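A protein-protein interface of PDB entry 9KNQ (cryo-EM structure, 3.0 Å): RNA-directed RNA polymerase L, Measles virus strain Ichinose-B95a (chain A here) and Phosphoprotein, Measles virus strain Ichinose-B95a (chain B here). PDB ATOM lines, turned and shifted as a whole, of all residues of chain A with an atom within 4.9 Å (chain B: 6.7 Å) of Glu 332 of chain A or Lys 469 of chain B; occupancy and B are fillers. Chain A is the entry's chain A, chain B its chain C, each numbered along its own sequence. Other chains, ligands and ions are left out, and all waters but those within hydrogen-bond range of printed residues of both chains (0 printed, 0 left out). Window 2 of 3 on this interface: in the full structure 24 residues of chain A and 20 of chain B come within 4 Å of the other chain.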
ATOM      1  N   HIS A 328      17.244  10.544  36.393  1.00  0.00           N
ATOM      2  CA  HIS A 328      17.883   9.376  35.798  1.00  0.00           C
ATOM      3  C   HIS A 328      17.327   9.089  34.408  1.00  0.00           C
ATOM      4  O   HIS A 328      18.087   8.836  33.462  1.00  0.00           O
ATOM      5  CB  HIS A 328      17.697   8.170  36.715  1.00  0.00           C
ATOM      6  CG  HIS A 328      18.541   6.992  36.344  1.00  0.00           C
ATOM      7  ND1 HIS A 328      18.093   5.986  35.517  1.00  0.00           N
ATOM      8  CD2 HIS A 328      19.805   6.657  36.695  1.00  0.00           C
ATOM      9  CE1 HIS A 328      19.045   5.082  35.372  1.00  0.00           C
ATOM     10  NE2 HIS A 328      20.094   5.466  36.076  1.00  0.00           N
ATOM     11  N   GLU A 329      16.002   9.138  34.261  1.00  0.00           N
ATOM     12  CA  GLU A 329      15.402   8.858  32.963  1.00  0.00           C
ATOM     13  C   GLU A 329      15.766   9.928  31.942  1.00  0.00           C
ATOM     14  O   GLU A 329      16.027   9.615  30.773  1.00  0.00           O
ATOM     15  CB  GLU A 329      13.888   8.734  33.105  1.00  0.00           C
ATOM     16  CG  GLU A 329      13.457   7.523  33.909  1.00  0.00           C
ATOM     17  CD  GLU A 329      11.970   7.257  33.815  1.00  0.00           C
ATOM     18  OE1 GLU A 329      11.465   6.423  34.596  1.00  0.00           O
ATOM     19  OE2 GLU A 329      11.306   7.881  32.961  1.00  0.00           O
ATOM     20  N   LEU A 330      15.797  11.193  32.363  1.00  0.00           N
ATOM     21  CA  LEU A 330      16.193  12.259  31.451  1.00  0.00           C
ATOM     22  C   LEU A 330      17.632  12.076  30.987  1.00  0.00           C
ATOM     23  O   LEU A 330      17.947  12.299  29.811  1.00  0.00           O
ATOM     24  CB  LEU A 330      16.010  13.616  32.125  1.00  0.00           C
ATOM     25  CG  LEU A 330      16.520  14.839  31.367  1.00  0.00           C
ATOM     26  CD1 LEU A 330      15.907  14.904  29.988  1.00  0.00           C
ATOM     27  CD2 LEU A 330      16.212  16.102  32.143  1.00  0.00           C
ATOM     28  N   ILE A 331      18.519  11.663  31.894  1.00  0.00           N
ATOM     29  CA  ILE A 331      19.910  11.441  31.512  1.00  0.00           C
ATOM     30  C   ILE A 331      20.014  10.293  30.519  1.00  0.00           C
ATOM     31  O   ILE A 331      20.764  10.368  29.537  1.00  0.00           O
ATOM     32  CB  ILE A 331      20.773  11.193  32.760  1.00  0.00           C
ATOM     33  CG1 ILE A 331      20.952  12.491  33.538  1.00  0.00           C
ATOM     34  CG2 ILE A 331      22.118  10.628  32.368  1.00  0.00           C
ATOM     35  CD1 ILE A 331      21.418  13.638  32.688  1.00  0.00           C
ATOM     36  N   GLU A 332      19.266   9.212  30.756  1.00  0.00           N
ATOM     37  CA  GLU A 332      19.268   8.102  29.805  1.00  0.00           C
ATOM     38  C   GLU A 332      18.790   8.553  28.430  1.00  0.00           C
ATOM     39  O   GLU A 332      19.371   8.176  27.401  1.00  0.00           O
ATOM     40  CB  GLU A 332      18.390   6.966  30.323  1.00  0.00           C
ATOM     41  CG  GLU A 332      18.909   6.299  31.578  1.00  0.00           C
ATOM     42  CD  GLU A 332      20.119   5.432  31.317  1.00  0.00           C
ATOM     43  OE1 GLU A 332      21.250   5.954  31.379  1.00  0.00           O
ATOM     44  OE2 GLU A 332      19.940   4.226  31.047  1.00  0.00           O
ATOM     45  N   ALA A 333      17.730   9.362  28.394  1.00  0.00           N
ATOM     46  CA  ALA A 333      17.213   9.843  27.118  1.00  0.00           C
ATOM     47  C   ALA A 333      18.237  10.707  26.397  1.00  0.00           C
ATOM     48  O   ALA A 333      18.432  10.566  25.184  1.00  0.00           O
ATOM     49  CB  ALA A 333      15.917  10.620  27.336  1.00  0.00           C
ATOM     50  N   LEU A 334      18.895  11.614  27.121  1.00  0.00           N
ATOM     51  CA  LEU A 334      19.902  12.460  26.488  1.00  0.00           C
ATOM     52  C   LEU A 334      21.061  11.630  25.958  1.00  0.00           C
ATOM     53  O   LEU A 334      21.599  11.914  24.879  1.00  0.00           O
ATOM     54  CB  LEU A 334      20.403  13.512  27.475  1.00  0.00           C
ATOM     55  CG  LEU A 334      19.470  14.693  27.722  1.00  0.00           C
ATOM     56  CD1 LEU A 334      20.134  15.706  28.625  1.00  0.00           C
ATOM     57  CD2 LEU A 334      19.073  15.330  26.414  1.00  0.00           C
ATOM     58  N   ASP A 335      21.467  10.605  26.709  1.00  0.00           N
ATOM     59  CA  ASP A 335      22.493   9.689  26.223  1.00  0.00           C
ATOM     60  C   ASP A 335      22.084   9.073  24.896  1.00  0.00           C
ATOM     61  O   ASP A 335      22.829   9.130  23.909  1.00  0.00           O
ATOM     62  CB  ASP A 335      22.754   8.599  27.260  1.00  0.00           C
ATOM     63  CG  ASP A 335      24.034   8.822  28.028  1.00  0.00           C
ATOM     64  OD1 ASP A 335      24.707   9.841  27.776  1.00  0.00           O
ATOM     65  OD2 ASP A 335      24.367   7.978  28.885  1.00  0.00           O
ATOM     66  N   TYR A 336      20.885   8.484  24.855  1.00  0.00           N
ATOM     67  CA  TYR A 336      20.428   7.840  23.627  1.00  0.00           C
ATOM     68  C   TYR A 336      20.358   8.828  22.472  1.00  0.00           C
ATOM     69  O   TYR A 336      20.649   8.475  21.325  1.00  0.00           O
ATOM     70  CB  TYR A 336      19.065   7.189  23.835  1.00  0.00           C
ATOM     71  CG  TYR A 336      18.407   6.797  22.535  1.00  0.00           C
ATOM     72  CD1 TYR A 336      18.923   5.775  21.759  1.00  0.00           C
ATOM     73  CD2 TYR A 336      17.281   7.458  22.079  1.00  0.00           C
ATOM     74  CE1 TYR A 336      18.331   5.416  20.570  1.00  0.00           C
ATOM     75  CE2 TYR A 336      16.682   7.105  20.890  1.00  0.00           C
ATOM     76  CZ  TYR A 336      17.212   6.083  20.140  1.00  0.00           C
ATOM     77  OH  TYR A 336      16.623   5.724  18.953  1.00  0.00           O
ATOM     78  N   ILE A 339      24.615  10.278  21.851  1.00  0.00           N
ATOM     79  CA  ILE A 339      25.753   9.390  21.624  1.00  0.00           C
ATOM     80  C   ILE A 339      25.653   8.795  20.226  1.00  0.00           C
ATOM     81  O   ILE A 339      24.658   8.148  19.879  1.00  0.00           O
ATOM     82  CB  ILE A 339      25.818   8.291  22.690  1.00  0.00           C
ATOM     83  CG1 ILE A 339      26.447   8.831  23.970  1.00  0.00           C
ATOM     84  CG2 ILE A 339      26.624   7.116  22.182  1.00  0.00           C
ATOM     85  CD1 ILE A 339      26.677   7.776  25.017  1.00  0.00           C
ATOM     86  N   ILE B 464      30.465   8.958  34.340  1.00  0.00           N
ATOM     87  CA  ILE B 464      31.223   7.720  34.187  1.00  0.00           C
ATOM     88  C   ILE B 464      30.464   6.741  33.300  1.00  0.00           C
ATOM     89  O   ILE B 464      31.048   6.088  32.424  1.00  0.00           O
ATOM     90  CB  ILE B 464      31.546   7.109  35.563  1.00  0.00           C
ATOM     91  CG1 ILE B 464      32.529   7.997  36.321  1.00  0.00           C
ATOM     92  CG2 ILE B 464      32.131   5.718  35.405  1.00  0.00           C
ATOM     93  CD1 ILE B 464      32.964   7.423  37.646  1.00  0.00           C
ATOM     94  N   ARG B 465      29.150   6.623  33.513  1.00  0.00           N
ATOM     95  CA  ARG B 465      28.340   5.774  32.646  1.00  0.00           C
ATOM     96  C   ARG B 465      28.426   6.229  31.196  1.00  0.00           C
ATOM     97  O   ARG B 465      28.509   5.403  30.282  1.00  0.00           O
ATOM     98  CB  ARG B 465      26.887   5.777  33.112  1.00  0.00           C
ATOM     99  CG  ARG B 465      26.629   4.993  34.376  1.00  0.00           C
ATOM    100  CD  ARG B 465      25.141   4.762  34.554  1.00  0.00           C
ATOM    101  NE  ARG B 465      24.816   4.275  35.889  1.00  0.00           N
ATOM    102  CZ  ARG B 465      23.602   3.882  36.262  1.00  0.00           C
ATOM    103  NH1 ARG B 465      22.599   3.918  35.397  1.00  0.00           N
ATOM    104  NH2 ARG B 465      23.391   3.453  37.499  1.00  0.00           N
ATOM    105  N   SER B 466      28.398   7.542  30.969  1.00  0.00           N
ATOM    106  CA  SER B 466      28.475   8.053  29.606  1.00  0.00           C
ATOM    107  C   SER B 466      29.823   7.738  28.975  1.00  0.00           C
ATOM    108  O   SER B 466      29.893   7.410  27.786  1.00  0.00           O
ATOM    109  CB  SER B 466      28.213   9.556  29.594  1.00  0.00           C
ATOM    110  OG  SER B 466      27.117   9.877  30.427  1.00  0.00           O
ATOM    111  N   ILE B 467      30.903   7.838  29.749  1.00  0.00           N
ATOM    112  CA  ILE B 467      32.217   7.463  29.231  1.00  0.00           C
ATOM    113  C   ILE B 467      32.226   5.994  28.833  1.00  0.00           C
ATOM    114  O   ILE B 467      32.705   5.624  27.752  1.00  0.00           O
ATOM    115  CB  ILE B 467      33.314   7.774  30.263  1.00  0.00           C
ATOM    116  CG1 ILE B 467      33.467   9.282  30.443  1.00  0.00           C
ATOM    117  CG2 ILE B 467      34.630   7.168  29.830  1.00  0.00           C
ATOM    118  CD1 ILE B 467      34.588   9.668  31.373  1.00  0.00           C
ATOM    119  N   ILE B 468      31.684   5.134  29.698  1.00  0.00           N
ATOM    120  CA  ILE B 468      31.651   3.705  29.394  1.00  0.00           C
ATOM    121  C   ILE B 468      30.848   3.446  28.126  1.00  0.00           C
ATOM    122  O   ILE B 468      31.251   2.650  27.270  1.00  0.00           O
ATOM    123  CB  ILE B 468      31.093   2.908  30.585  1.00  0.00           C
ATOM    124  CG1 ILE B 468      31.956   3.123  31.822  1.00  0.00           C
ATOM    125  CG2 ILE B 468      31.042   1.436  30.248  1.00  0.00           C
ATOM    126  CD1 ILE B 468      31.443   2.406  33.042  1.00  0.00           C
ATOM    127  N   LYS B 469      29.702   4.115  27.984  1.00  0.00           N
ATOM    128  CA  LYS B 469      28.861   3.908  26.808  1.00  0.00           C
ATOM    129  C   LYS B 469      29.550   4.386  25.539  1.00  0.00           C
ATOM    130  O   LYS B 469      29.499   3.709  24.506  1.00  0.00           O
ATOM    131  CB  LYS B 469      27.526   4.627  26.980  1.00  0.00           C
ATOM    132  CG  LYS B 469      26.569   3.961  27.943  1.00  0.00           C
ATOM    133  CD  LYS B 469      25.265   4.733  28.010  1.00  0.00           C
ATOM    134  CE  LYS B 469      24.304   4.118  29.004  1.00  0.00           C
ATOM    135  NZ  LYS B 469      23.053   4.912  29.097  1.00  0.00           N
ATOM    136  N   SER B 470      30.192   5.550  25.589  1.00  0.00           N
ATOM    137  CA  SER B 470      30.845   6.105  24.414  1.00  0.00           C
ATOM    138  C   SER B 470      32.218   5.507  24.157  1.00  0.00           C
ATOM    139  O   SER B 470      32.868   5.893  23.181  1.00  0.00           O
ATOM    140  CB  SER B 470      30.973   7.620  24.549  1.00  0.00           C
ATOM    141  OG  SER B 470      31.954   8.113  23.657  1.00  0.00           O
ATOM    142  N   SER B 471      32.673   4.580  24.995  1.00  0.00           N
ATOM    143  CA  SER B 471      33.954   3.933  24.766  1.00  0.00           C
ATOM    144  C   SER B 471      33.882   3.031  23.534  1.00  0.00           C
ATOM    145  O   SER B 471      32.853   2.916  22.866  1.00  0.00           O
ATOM    146  CB  SER B 471      34.367   3.133  25.996  1.00  0.00           C
ATOM    147  OG  SER B 471      33.976   3.803  27.180  1.00  0.00           O
ATOM    148  N   ARG B 472      35.006   2.382  23.232  1.00  0.00           N
ATOM    149  CA  ARG B 472      35.118   1.500  22.075  1.00  0.00           C
ATOM    150  C   ARG B 472      35.311   0.045  22.483  1.00  0.00           C
ATOM    151  O   ARG B 472      35.864  -0.745  21.712  1.00  0.00           O
ATOM    152  CB  ARG B 472      36.266   1.950  21.171  1.00  0.00           C
ATOM    153  CG  ARG B 472      35.831   2.759  19.967  1.00  0.00           C
ATOM    154  CD  ARG B 472      36.891   2.710  18.880  1.00  0.00           C
ATOM    155  NE  ARG B 472      36.531   3.518  17.720  1.00  0.00           N
ATOM    156  CZ  ARG B 472      37.262   3.598  16.614  1.00  0.00           C
ATOM    157  NH1 ARG B 472      38.396   2.918  16.517  1.00  0.00           N
ATOM    158  NH2 ARG B 472      36.862   4.360  15.605  1.00  0.00           N
ATOM    159  N   LYS B 478      31.206  -3.670  28.556  1.00  0.00           N
ATOM    160  CA  LYS B 478      30.474  -2.521  29.078  1.00  0.00           C
ATOM    161  C   LYS B 478      29.477  -2.953  30.144  1.00  0.00           C
ATOM    162  O   LYS B 478      29.322  -2.282  31.172  1.00  0.00           O
ATOM    163  CB  LYS B 478      29.760  -1.794  27.939  1.00  0.00           C
ATOM    164  CG  LYS B 478      30.692  -1.223  26.888  1.00  0.00           C
ATOM    165  CD  LYS B 478      29.918  -0.662  25.709  1.00  0.00           C
ATOM    166  CE  LYS B 478      30.845  -0.328  24.555  1.00  0.00           C
ATOM    167  NZ  LYS B 478      30.091   0.087  23.343  1.00  0.00           N
ATOM    168  N   MET B 482      29.488  -1.729  34.036  1.00  0.00           N
ATOM    169  CA  MET B 482      28.308  -1.155  34.675  1.00  0.00           C
ATOM    170  C   MET B 482      27.919  -1.942  35.920  1.00  0.00           C
ATOM    171  O   MET B 482      27.509  -1.359  36.933  1.00  0.00           O
ATOM    172  CB  MET B 482      27.143  -1.109  33.690  1.00  0.00           C
ATOM    173  CG  MET B 482      27.282  -0.058  32.607  1.00  0.00           C
ATOM    174  SD  MET B 482      26.673   1.557  33.123  1.00  0.00           S
ATOM    175  CE  MET B 482      24.924   1.223  33.318  1.00  0.00           C
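Printed residues of chain B that touch a printed residue of chain A: Arg 465, Ser 466 and Lys 469. Hydrophobic or aromatic side chains of chain A within 4 Å of the printed part of chain B: His 328 and Ile 339. Among the printed residues, 5 pairs touch across the chains. Among the printed residues, Asp or Glu carboxylates within 4 Å of a Lys or Arg side-chain nitrogen of the other chain: Glu 332 of chain A with Lys 469 of chain B (3.1 Å) and Asp 335 of chain A with Lys 469 of chain B (3.3 Å).
Of the printed residues of chain B, His 328 of chain A touches Arg 465. Glu 332 of chain A touches just one residue of chain B: Lys 469 (3.1 Å). Printed residues of chain B within 4 Å of Asp 335 of chain A: Ser 466 (3.6 Å) and Lys 469 (3.3 Å). Of the printed residues of chain B, Ile 339 of chain A touches Lys 469. Lys 469 of chain B touches just these residues of chain A: Glu 332, Asp 335 and Ile 339. The nearest residue of chain B that does not touch Glu 332 of chain A is Arg 465 of chain B (4.7 Å). The nearest printed residue of chain B that does not touch Asp 335 of chain A is Arg 465 of chain B (5.0 Å).
The side-chain carboxylate of Glu 332 of chain A lies within salt-bridge range of the side-chain amino group of Lys 469 of chain B, 3.1 Å away. NH1 of Arg 465 of chain B is in hydrogen-bond range of NE2 of His 328 of chain A (3.0 Å). NZ of Lys 469 of chain B lies within salt-bridge range of OD2 of Asp 335 of chain A (3.3 Å).
Among the printed residues, pairs that only touch across the chains: Asp 335 of chain A with Ser 466 of chain B (3.6 Å) and Ile 339 of chain A with Lys 469 of chain B (3.8 Å).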
